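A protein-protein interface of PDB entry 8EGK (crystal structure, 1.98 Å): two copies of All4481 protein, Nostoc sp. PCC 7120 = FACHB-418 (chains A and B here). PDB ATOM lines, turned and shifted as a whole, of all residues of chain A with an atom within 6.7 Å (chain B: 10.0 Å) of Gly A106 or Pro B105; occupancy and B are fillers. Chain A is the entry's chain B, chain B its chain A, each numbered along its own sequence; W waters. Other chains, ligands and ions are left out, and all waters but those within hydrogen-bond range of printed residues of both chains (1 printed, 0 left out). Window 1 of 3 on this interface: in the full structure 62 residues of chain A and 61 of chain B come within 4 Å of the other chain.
The guanidinium group (NE) of Arg B140 lies within salt-bridge range of the side-chain carboxylate (OD2) of Asp A108 (3.7 Å).
Hydrophobic or aromatic side chains of chain A that line the printed part of chain B: Val A103, Pro A105, Phe A137, Leu A144 and Leu A148.
Of the 18 printed residues of chain B, 11 touch a printed residue of chain A.
Among the printed residues, 19 pairs touch across the chains.
Among the printed residues, Asp or Glu carboxylates within 4 Å of a Lys or Arg side-chain nitrogen of the other chain: Asp A108 with Arg B140 (3.7 Å).
Water W1 lies within hydrogen-bond range of the side-chain hydroxyl of Ser A147, the backbone carbonyl oxygen of Arg A140 and the backbone carbonyl oxygen of Val B103.
The backbone NH (N) of Leu B104 sits at hydrogen-bond distance from the side-chain sulfur (SD) of Met B107 (3.6 Å).
The backbone NH (N) of Gly A106 is in hydrogen-bond range of the side-chain carboxylate (OD1) of Asp A108, at 2.8 Å.
The backbone carbonyl oxygen of Gly A143 sits at hydrogen-bond distance from the side-chain hydroxyl of Ser A147.
OD1 of Asp B108 sits at hydrogen-bond distance from N of Gly B106 (2.8 Å).
Arg B140 touches Val A103 (NE to CG1, 3.4 Å).
Pro A105 touches Leu B144 (CD to CD2, 3.6 Å).
Pro B105 touches Gly A106.
Asp A108 touches Phe B137.
Ser A109 touches Pro B105.
CD2 of Phe B137 touches CD2 of Phe A137, at 3.4 Å.
Ser B69 touches Arg A140 (CB to NH2, 3.7 Å).
Arg A140 touches Val B103 (NE to CG1, 3.2 Å).
Pro B105 touches Arg A140 (CG to O, 3.5 Å).
Ser A147 touches Val B102 (OG to CG1, 3.3 Å).
Printed residues of chain B within 4 Å of Val A103: Arg B140 (3.4 Å).
Pro A105 touches just these residues of chain B: Gly B106, Ser B109, Arg B140 and Leu B144.
Gly A106 touches two residues of chain B.
Leu A142 touches none of the printed residues of chain B.
Printed residues of chain A within 4 Å of Ser B69: Arg A140 (3.7 Å).
Pro B105 touches four residues of chain A.
Printed residues of chain A within 4 Å of Gly B106: Pro A105 (3.4 Å) and Gly A106 (3.3 Å).
Ala B110 touches none of the printed residues of chain A.
Printed residues of chain A within 4 Å of Arg B140: Val A103 (3.4 Å), Pro A105 (3.6 Å) and Asp A108 (3.7 Å).
The nearest printed residue of chain B that does not touch Gly A106 is Asp B108 (5.6 Å).
The nearest printed residue of chain B that does not touch Val A103 is Leu B144 (6.8 Å).
Val A103 touches Arg B140, and with the chains exchanged Arg A140 touches Val B103.
Pro A105 touches Arg B140, and with the chains exchanged Arg A140 touches Pro B105.
Asp A108 touches Phe B137, and with the chains exchanged Phe A137 touches Asp B108.
Phe A137 touches its own counterpart, Phe B137.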
ATOM      1  N   VAL A 103     -26.041   4.542 -33.888  1.00  0.00           N
ATOM      2  CA  VAL A 103     -25.981   3.346 -33.056  1.00  0.00           C
ATOM      3  C   VAL A 103     -26.116   3.764 -31.599  1.00  0.00           C
ATOM      4  O   VAL A 103     -25.302   4.530 -31.090  1.00  0.00           O
ATOM      5  CB  VAL A 103     -24.674   2.584 -33.304  1.00  0.00           C
ATOM      6  CG1 VAL A 103     -24.478   1.473 -32.290  1.00  0.00           C
ATOM      7  CG2 VAL A 103     -24.641   2.040 -34.720  1.00  0.00           C
ATOM      8  N   LEU A 104     -27.166   3.273 -30.920  1.00  0.00           N
ATOM      9  CA  LEU A 104     -27.248   3.544 -29.489  1.00  0.00           C
ATOM     10  C   LEU A 104     -26.561   2.442 -28.687  1.00  0.00           C
ATOM     11  O   LEU A 104     -26.282   1.367 -29.206  1.00  0.00           O
ATOM     12  CB  LEU A 104     -28.706   3.659 -29.064  1.00  0.00           C
ATOM     13  CG  LEU A 104     -29.514   4.791 -29.706  1.00  0.00           C
ATOM     14  CD1 LEU A 104     -30.999   4.468 -29.611  1.00  0.00           C
ATOM     15  CD2 LEU A 104     -29.195   6.123 -29.050  1.00  0.00           C
ATOM     16  N   PRO A 105     -26.274   2.676 -27.410  1.00  0.00           N
ATOM     17  CA  PRO A 105     -25.804   1.575 -26.563  1.00  0.00           C
ATOM     18  C   PRO A 105     -26.793   0.419 -26.602  1.00  0.00           C
ATOM     19  O   PRO A 105     -28.007   0.622 -26.644  1.00  0.00           O
ATOM     20  CB  PRO A 105     -25.717   2.208 -25.169  1.00  0.00           C
ATOM     21  CG  PRO A 105     -25.545   3.688 -25.429  1.00  0.00           C
ATOM     22  CD  PRO A 105     -26.330   3.962 -26.684  1.00  0.00           C
ATOM     23  N   GLY A 106     -26.264  -0.798 -26.604  1.00  0.00           N
ATOM     24  CA  GLY A 106     -27.074  -2.019 -26.619  1.00  0.00           C
ATOM     25  C   GLY A 106     -27.347  -2.498 -28.008  1.00  0.00           C
ATOM     26  O   GLY A 106     -27.267  -3.690 -28.306  1.00  0.00           O
ATOM     27  N   MET A 107     -27.669  -1.562 -28.886  1.00  0.00           N
ATOM     28  CA  MET A 107     -27.786  -1.796 -30.308  1.00  0.00           C
ATOM     29  C   MET A 107     -26.483  -2.339 -30.850  1.00  0.00           C
ATOM     30  O   MET A 107     -26.478  -3.284 -31.635  1.00  0.00           O
ATOM     31  CB  MET A 107     -28.200  -0.447 -30.918  1.00  0.00           C
ATOM     32  CG  MET A 107     -28.190  -0.286 -32.366  1.00  0.00           C
ATOM     33  SD  MET A 107     -29.482   1.183 -32.747  1.00  0.00           S
ATOM     34  CE  MET A 107     -30.662   1.323 -31.322  1.00  0.00           C
ATOM     35  N   ASP A 108     -25.359  -1.785 -30.386  1.00  0.00           N
ATOM     36  CA  ASP A 108     -24.064  -2.267 -30.862  1.00  0.00           C
ATOM     37  C   ASP A 108     -23.878  -3.753 -30.556  1.00  0.00           C
ATOM     38  O   ASP A 108     -23.404  -4.518 -31.403  1.00  0.00           O
ATOM     39  CB  ASP A 108     -22.931  -1.443 -30.238  1.00  0.00           C
ATOM     40  CG  ASP A 108     -23.156  -1.141 -28.763  1.00  0.00           C
ATOM     41  OD1 ASP A 108     -24.067  -1.745 -28.136  1.00  0.00           O
ATOM     42  OD2 ASP A 108     -22.412  -0.300 -28.217  1.00  0.00           O
ATOM     43  N   SER A 109     -24.281  -4.181 -29.359  1.00  0.00           N
ATOM     44  CA  SER A 109     -24.111  -5.572 -28.953  1.00  0.00           C
ATOM     45  C   SER A 109     -25.097  -6.504 -29.663  1.00  0.00           C
ATOM     46  O   SER A 109     -24.735  -7.630 -30.049  1.00  0.00           O
ATOM     47  CB  SER A 109     -24.278  -5.666 -27.439  1.00  0.00           C
ATOM     48  OG  SER A 109     -23.148  -5.102 -26.794  1.00  0.00           O
ATOM     49  N   ALA A 110     -26.342  -6.067 -29.843  1.00  0.00           N
ATOM     50  CA  ALA A 110     -27.313  -6.894 -30.551  1.00  0.00           C
ATOM     51  C   ALA A 110     -26.907  -7.086 -32.009  1.00  0.00           C
ATOM     52  O   ALA A 110     -27.013  -8.195 -32.553  1.00  0.00           O
ATOM     53  CB  ALA A 110     -28.705  -6.268 -30.452  1.00  0.00           C
ATOM     54  N   LEU A 111     -26.428  -6.021 -32.651  1.00  0.00           N
ATOM     55  CA  LEU A 111     -26.016  -6.118 -34.048  1.00  0.00           C
ATOM     56  C   LEU A 111     -24.861  -7.094 -34.204  1.00  0.00           C
ATOM     57  O   LEU A 111     -24.858  -7.921 -35.121  1.00  0.00           O
ATOM     58  CB  LEU A 111     -25.622  -4.733 -34.566  1.00  0.00           C
ATOM     59  CG  LEU A 111     -26.748  -3.735 -34.827  1.00  0.00           C
ATOM     60  CD1 LEU A 111     -26.209  -2.297 -34.747  1.00  0.00           C
ATOM     61  CD2 LEU A 111     -27.421  -3.974 -36.177  1.00  0.00           C
ATOM     62  N   PHE A 137     -19.424  -6.458 -20.509  1.00  0.00           N
ATOM     63  CA  PHE A 137     -20.260  -6.071 -21.636  1.00  0.00           C
ATOM     64  C   PHE A 137     -20.340  -7.193 -22.663  1.00  0.00           C
ATOM     65  O   PHE A 137     -21.387  -7.400 -23.288  1.00  0.00           O
ATOM     66  CB  PHE A 137     -19.727  -4.786 -22.275  1.00  0.00           C
ATOM     67  CG  PHE A 137     -19.851  -3.566 -21.391  1.00  0.00           C
ATOM     68  CD1 PHE A 137     -19.258  -3.532 -20.132  1.00  0.00           C
ATOM     69  CD2 PHE A 137     -20.555  -2.458 -21.824  1.00  0.00           C
ATOM     70  CE1 PHE A 137     -19.376  -2.409 -19.316  1.00  0.00           C
ATOM     71  CE2 PHE A 137     -20.673  -1.331 -21.021  1.00  0.00           C
ATOM     72  CZ  PHE A 137     -20.084  -1.308 -19.766  1.00  0.00           C
ATOM     73  N   ARG A 140     -22.942  -9.537 -21.180  1.00  0.00           N
ATOM     74  CA  ARG A 140     -24.335  -9.126 -21.345  1.00  0.00           C
ATOM     75  C   ARG A 140     -24.808  -9.365 -22.768  1.00  0.00           C
ATOM     76  O   ARG A 140     -25.977  -9.693 -22.998  1.00  0.00           O
ATOM     77  CB  ARG A 140     -24.494  -7.662 -20.966  1.00  0.00           C
ATOM     78  CG  ARG A 140     -24.342  -7.449 -19.478  1.00  0.00           C
ATOM     79  CD  ARG A 140     -25.493  -6.667 -18.919  1.00  0.00           C
ATOM     80  NE  ARG A 140     -25.087  -5.942 -17.724  1.00  0.00           N
ATOM     81  CZ  ARG A 140     -25.063  -6.459 -16.505  1.00  0.00           C
ATOM     82  NH1 ARG A 140     -25.440  -7.708 -16.280  1.00  0.00           N
ATOM     83  NH2 ARG A 140     -24.668  -5.702 -15.485  1.00  0.00           N
ATOM     84  N   MET A 141     -23.923  -9.190 -23.733  1.00  0.00           N
ATOM     85  CA  MET A 141     -24.228  -9.564 -25.102  1.00  0.00           C
ATOM     86  C   MET A 141     -24.496 -11.048 -25.290  1.00  0.00           C
ATOM     87  O   MET A 141     -25.570 -11.442 -25.791  1.00  0.00           O
ATOM     88  CB  MET A 141     -23.068  -9.163 -26.021  1.00  0.00           C
ATOM     89  CG  MET A 141     -23.440  -9.217 -27.458  1.00  0.00           C
ATOM     90  SD  MET A 141     -21.886  -9.211 -28.564  1.00  0.00           S
ATOM     91  CE  MET A 141     -20.781 -10.595 -27.734  1.00  0.00           C
ATOM     92  N   LEU A 142     -23.514 -11.880 -24.922  1.00  0.00           N
ATOM     93  CA  LEU A 142     -23.694 -13.321 -25.085  1.00  0.00           C
ATOM     94  C   LEU A 142     -24.942 -13.810 -24.364  1.00  0.00           C
ATOM     95  O   LEU A 142     -25.581 -14.766 -24.815  1.00  0.00           O
ATOM     96  CB  LEU A 142     -22.461 -14.071 -24.580  1.00  0.00           C
ATOM     97  CG  LEU A 142     -21.187 -13.850 -25.391  1.00  0.00           C
ATOM     98  CD1 LEU A 142     -19.987 -14.458 -24.665  1.00  0.00           C
ATOM     99  CD2 LEU A 142     -21.331 -14.412 -26.785  1.00  0.00           C
ATOM    100  N   GLY A 143     -25.307 -13.168 -23.260  1.00  0.00           N
ATOM    101  CA  GLY A 143     -26.478 -13.542 -22.494  1.00  0.00           C
ATOM    102  C   GLY A 143     -27.806 -13.071 -23.053  1.00  0.00           C
ATOM    103  O   GLY A 143     -28.855 -13.306 -22.438  1.00  0.00           O
ATOM    104  N   LEU A 144     -27.792 -12.413 -24.201  1.00  0.00           N
ATOM    105  CA  LEU A 144     -29.027 -11.864 -24.758  1.00  0.00           C
ATOM    106  C   LEU A 144     -30.120 -12.909 -24.938  1.00  0.00           C
ATOM    107  O   LEU A 144     -31.275 -12.639 -24.565  1.00  0.00           O
ATOM    108  CB  LEU A 144     -28.726 -11.188 -26.094  1.00  0.00           C
ATOM    109  CG  LEU A 144     -28.469  -9.689 -26.038  1.00  0.00           C
ATOM    110  CD1 LEU A 144     -27.782  -9.222 -27.318  1.00  0.00           C
ATOM    111  CD2 LEU A 144     -29.775  -8.952 -25.811  1.00  0.00           C
ATOM    112  N   SER A 147     -31.698 -13.488 -21.492  1.00  0.00           N
ATOM    113  CA  SER A 147     -32.290 -12.283 -20.930  1.00  0.00           C
ATOM    114  C   SER A 147     -33.567 -11.910 -21.671  1.00  0.00           C
ATOM    115  O   SER A 147     -34.571 -11.549 -21.050  1.00  0.00           O
ATOM    116  CB  SER A 147     -31.270 -11.143 -20.990  1.00  0.00           C
ATOM    117  OG  SER A 147     -30.087 -11.515 -20.328  1.00  0.00           O
ATOM    118  N   LEU A 148     -33.539 -11.986 -22.994  1.00  0.00           N
ATOM    119  CA  LEU A 148     -34.733 -11.714 -23.787  1.00  0.00           C
ATOM    120  C   LEU A 148     -35.817 -12.750 -23.509  1.00  0.00           C
ATOM    121  O   LEU A 148     -36.983 -12.401 -23.303  1.00  0.00           O
ATOM    122  CB  LEU A 148     -34.374 -11.693 -25.274  1.00  0.00           C
ATOM    123  CG  LEU A 148     -33.362 -10.619 -25.686  1.00  0.00           C
ATOM    124  CD1 LEU A 148     -33.217 -10.550 -27.192  1.00  0.00           C
ATOM    125  CD2 LEU A 148     -33.734  -9.255 -25.128  1.00  0.00           C
ATOM    126  N   SER B  69     -25.398  -2.217 -12.043  1.00  0.00           N
ATOM    127  CA  SER B  69     -26.565  -2.063 -12.916  1.00  0.00           C
ATOM    128  C   SER B  69     -27.805  -2.756 -12.351  1.00  0.00           C
ATOM    129  O   SER B  69     -28.929  -2.281 -12.557  1.00  0.00           O
ATOM    130  CB  SER B  69     -26.261  -2.593 -14.310  1.00  0.00           C
ATOM    131  OG  SER B  69     -25.101  -1.986 -14.838  1.00  0.00           O
ATOM    132  N   LEU B  73     -31.053  -0.569 -11.871  1.00  0.00           N
ATOM    133  CA  LEU B  73     -32.262  -1.001 -12.562  1.00  0.00           C
ATOM    134  C   LEU B  73     -33.439  -1.108 -11.590  1.00  0.00           C
ATOM    135  O   LEU B  73     -34.534  -0.598 -11.865  1.00  0.00           O
ATOM    136  CB  LEU B  73     -31.998  -2.332 -13.270  1.00  0.00           C
ATOM    137  CG  LEU B  73     -33.137  -2.928 -14.085  1.00  0.00           C
ATOM    138  CD1 LEU B  73     -33.765  -1.885 -14.977  1.00  0.00           C
ATOM    139  CD2 LEU B  73     -32.628  -4.123 -14.905  1.00  0.00           C
ATOM    140  N   VAL B 102     -33.591  -8.319 -15.364  1.00  0.00           N
ATOM    141  CA  VAL B 102     -32.306  -8.704 -15.931  1.00  0.00           C
ATOM    142  C   VAL B 102     -31.769  -7.536 -16.744  1.00  0.00           C
ATOM    143  O   VAL B 102     -32.491  -6.940 -17.555  1.00  0.00           O
ATOM    144  CB  VAL B 102     -32.441  -9.969 -16.794  1.00  0.00           C
ATOM    145  CG1 VAL B 102     -31.108 -10.345 -17.417  1.00  0.00           C
ATOM    146  CG2 VAL B 102     -32.993 -11.116 -15.944  1.00  0.00           C
ATOM    147  N   VAL B 103     -30.496  -7.225 -16.546  1.00  0.00           N
ATOM    148  CA  VAL B 103     -29.867  -6.107 -17.238  1.00  0.00           C
ATOM    149  C   VAL B 103     -29.612  -6.513 -18.682  1.00  0.00           C
ATOM    150  O   VAL B 103     -28.993  -7.551 -18.955  1.00  0.00           O
ATOM    151  CB  VAL B 103     -28.568  -5.695 -16.527  1.00  0.00           C
ATOM    152  CG1 VAL B 103     -27.927  -4.504 -17.236  1.00  0.00           C
ATOM    153  CG2 VAL B 103     -28.858  -5.364 -15.052  1.00  0.00           C
ATOM    154  N   LEU B 104     -30.131  -5.722 -19.613  1.00  0.00           N
ATOM    155  CA  LEU B 104     -29.897  -5.916 -21.033  1.00  0.00           C
ATOM    156  C   LEU B 104     -28.781  -5.003 -21.519  1.00  0.00           C
ATOM    157  O   LEU B 104     -28.525  -3.947 -20.926  1.00  0.00           O
ATOM    158  CB  LEU B 104     -31.173  -5.619 -21.833  1.00  0.00           C
ATOM    159  CG  LEU B 104     -32.401  -6.504 -21.578  1.00  0.00           C
ATOM    160  CD1 LEU B 104     -33.552  -6.078 -22.489  1.00  0.00           C
ATOM    161  CD2 LEU B 104     -32.084  -7.970 -21.788  1.00  0.00           C
ATOM    162  N   PRO B 105     -28.108  -5.364 -22.614  1.00  0.00           N
ATOM    163  CA  PRO B 105     -27.148  -4.440 -23.227  1.00  0.00           C
ATOM    164  C   PRO B 105     -27.792  -3.090 -23.475  1.00  0.00           C
ATOM    165  O   PRO B 105     -28.973  -3.003 -23.828  1.00  0.00           O
ATOM    166  CB  PRO B 105     -26.779  -5.134 -24.552  1.00  0.00           C
ATOM    167  CG  PRO B 105     -27.006  -6.576 -24.274  1.00  0.00           C
ATOM    168  CD  PRO B 105     -28.177  -6.643 -23.333  1.00  0.00           C
ATOM    169  N   GLY B 106     -27.008  -2.036 -23.312  1.00  0.00           N
ATOM    170  CA  GLY B 106     -27.497  -0.674 -23.449  1.00  0.00           C
ATOM    171  C   GLY B 106     -28.033  -0.135 -22.138  1.00  0.00           C
ATOM    172  O   GLY B 106     -27.768   1.019 -21.784  1.00  0.00           O
ATOM    173  N   MET B 107     -28.776  -0.962 -21.395  1.00  0.00           N
ATOM    174  CA  MET B 107     -29.283  -0.545 -20.095  1.00  0.00           C
ATOM    175  C   MET B 107     -28.140  -0.166 -19.187  1.00  0.00           C
ATOM    176  O   MET B 107     -28.227   0.789 -18.413  1.00  0.00           O
ATOM    177  CB  MET B 107     -30.079  -1.639 -19.406  1.00  0.00           C
ATOM    178  CG  MET B 107     -31.535  -1.668 -19.749  1.00  0.00           C
ATOM    179  SD  MET B 107     -32.392  -3.064 -18.625  1.00  0.00           S
ATOM    180  CE  MET B 107     -33.756  -3.542 -19.926  1.00  0.00           C
ATOM    181  N   ASP B 108     -27.063  -0.955 -19.266  1.00  0.00           N
ATOM    182  CA  ASP B 108     -25.889  -0.689 -18.443  1.00  0.00           C
ATOM    183  C   ASP B 108     -25.431   0.758 -18.607  1.00  0.00           C
ATOM    184  O   ASP B 108     -25.283   1.490 -17.630  1.00  0.00           O
ATOM    185  CB  ASP B 108     -24.780  -1.689 -18.806  1.00  0.00           C
ATOM    186  CG  ASP B 108     -24.745  -2.033 -20.306  1.00  0.00           C
ATOM    187  OD1 ASP B 108     -25.360  -1.297 -21.116  1.00  0.00           O
ATOM    188  OD2 ASP B 108     -24.135  -3.074 -20.679  1.00  0.00           O
ATOM    189  N   SER B 109     -25.244   1.195 -19.850  1.00  0.00           N
ATOM    190  CA  SER B 109     -24.762   2.547 -20.106  1.00  0.00           C
ATOM    191  C   SER B 109     -25.816   3.596 -19.785  1.00  0.00           C
ATOM    192  O   SER B 109     -25.485   4.653 -19.258  1.00  0.00           O
ATOM    193  CB  SER B 109     -24.326   2.671 -21.574  1.00  0.00           C
ATOM    194  OG  SER B 109     -23.225   1.815 -21.818  1.00  0.00           O
ATOM    195  N   ALA B 110     -27.081   3.343 -20.135  1.00  0.00           N
ATOM    196  CA  ALA B 110     -28.125   4.321 -19.856  1.00  0.00           C
ATOM    197  C   ALA B 110     -28.267   4.544 -18.358  1.00  0.00           C
ATOM    198  O   ALA B 110     -28.382   5.685 -17.901  1.00  0.00           O
ATOM    199  CB  ALA B 110     -29.463   3.874 -20.441  1.00  0.00           C
ATOM    200  N   LEU B 111     -28.272   3.457 -17.585  1.00  0.00           N
ATOM    201  CA  LEU B 111     -28.407   3.561 -16.137  1.00  0.00           C
ATOM    202  C   LEU B 111     -27.226   4.288 -15.521  1.00  0.00           C
ATOM    203  O   LEU B 111     -27.396   5.082 -14.589  1.00  0.00           O
ATOM    204  CB  LEU B 111     -28.524   2.166 -15.538  1.00  0.00           C
ATOM    205  CG  LEU B 111     -29.845   1.435 -15.808  1.00  0.00           C
ATOM    206  CD1 LEU B 111     -29.582  -0.077 -15.687  1.00  0.00           C
ATOM    207  CD2 LEU B 111     -30.951   1.877 -14.869  1.00  0.00           C
ATOM    208  N   ALA B 136     -14.754   2.375 -26.758  1.00  0.00           N
ATOM    209  CA  ALA B 136     -15.829   2.861 -27.620  1.00  0.00           C
ATOM    210  C   ALA B 136     -17.203   2.739 -26.977  1.00  0.00           C
ATOM    211  O   ALA B 136     -18.122   3.461 -27.379  1.00  0.00           O
ATOM    212  CB  ALA B 136     -15.828   2.089 -28.951  1.00  0.00           C
ATOM    213  N   PHE B 137     -17.381   1.837 -26.009  1.00  0.00           N
ATOM    214  CA  PHE B 137     -18.663   1.772 -25.302  1.00  0.00           C
ATOM    215  C   PHE B 137     -18.861   2.995 -24.423  1.00  0.00           C
ATOM    216  O   PHE B 137     -19.984   3.488 -24.266  1.00  0.00           O
ATOM    217  CB  PHE B 137     -18.743   0.511 -24.436  1.00  0.00           C
ATOM    218  CG  PHE B 137     -18.778  -0.765 -25.211  1.00  0.00           C
ATOM    219  CD1 PHE B 137     -19.023  -0.779 -26.570  1.00  0.00           C
ATOM    220  CD2 PHE B 137     -18.556  -1.975 -24.561  1.00  0.00           C
ATOM    221  CE1 PHE B 137     -19.045  -1.976 -27.279  1.00  0.00           C
ATOM    222  CE2 PHE B 137     -18.578  -3.170 -25.255  1.00  0.00           C
ATOM    223  CZ  PHE B 137     -18.818  -3.172 -26.617  1.00  0.00           C
ATOM    224  N   THR B 138     -17.781   3.482 -23.814  1.00  0.00           N
ATOM    225  CA  THR B 138     -17.860   4.716 -23.046  1.00  0.00           C
ATOM    226  C   THR B 138     -18.266   5.876 -23.937  1.00  0.00           C
ATOM    227  O   THR B 138     -19.093   6.710 -23.549  1.00  0.00           O
ATOM    228  CB  THR B 138     -16.525   4.986 -22.357  1.00  0.00           C
ATOM    229  OG1 THR B 138     -16.246   3.911 -21.460  1.00  0.00           O
ATOM    230  CG2 THR B 138     -16.547   6.271 -21.548  1.00  0.00           C
ATOM    231  N   ARG B 140     -20.063   5.750 -26.692  1.00  0.00           N
ATOM    232  CA  ARG B 140     -21.480   5.617 -27.052  1.00  0.00           C
ATOM    233  C   ARG B 140     -22.381   6.000 -25.891  1.00  0.00           C
ATOM    234  O   ARG B 140     -23.465   6.570 -26.096  1.00  0.00           O
ATOM    235  CB  ARG B 140     -21.759   4.189 -27.493  1.00  0.00           C
ATOM    236  CG  ARG B 140     -21.249   3.880 -28.873  1.00  0.00           C
ATOM    237  CD  ARG B 140     -22.271   3.068 -29.666  1.00  0.00           C
ATOM    238  NE  ARG B 140     -21.591   2.329 -30.714  1.00  0.00           N
ATOM    239  CZ  ARG B 140     -21.122   2.865 -31.832  1.00  0.00           C
ATOM    240  NH1 ARG B 140     -21.424   4.114 -32.185  1.00  0.00           N
ATOM    241  NH2 ARG B 140     -20.352   2.128 -32.622  1.00  0.00           N
ATOM    242  N   MET B 141     -21.958   5.707 -24.671  1.00  0.00           N
ATOM    243  CA  MET B 141     -22.646   6.218 -23.496  1.00  0.00           C
ATOM    244  C   MET B 141     -22.708   7.740 -23.458  1.00  0.00           C
ATOM    245  O   MET B 141     -23.786   8.337 -23.328  1.00  0.00           O
ATOM    246  CB  MET B 141     -21.928   5.821 -22.213  1.00  0.00           C
ATOM    247  CG  MET B 141     -22.698   6.238 -20.979  1.00  0.00           C
ATOM    248  SD  MET B 141     -21.887   5.456 -19.384  1.00  0.00           S
ATOM    249  CE  MET B 141     -20.621   6.755 -18.979  1.00  0.00           C
ATOM    250  N   LEU B 144     -24.973   9.661 -25.708  1.00  0.00           N
ATOM    251  CA  LEU B 144     -26.411   9.435 -25.654  1.00  0.00           C
ATOM    252  C   LEU B 144     -27.230  10.707 -25.812  1.00  0.00           C
ATOM    253  O   LEU B 144     -28.231  10.679 -26.539  1.00  0.00           O
ATOM    254  CB  LEU B 144     -26.804   8.757 -24.335  1.00  0.00           C
ATOM    255  CG  LEU B 144     -26.782   7.241 -24.353  1.00  0.00           C
ATOM    256  CD1 LEU B 144     -26.844   6.719 -22.952  1.00  0.00           C
ATOM    257  CD2 LEU B 144     -27.943   6.747 -25.185  1.00  0.00           C
HETATM  258  O   HOH W   1     -28.297  -9.630 -21.395  1.00  0.00           O
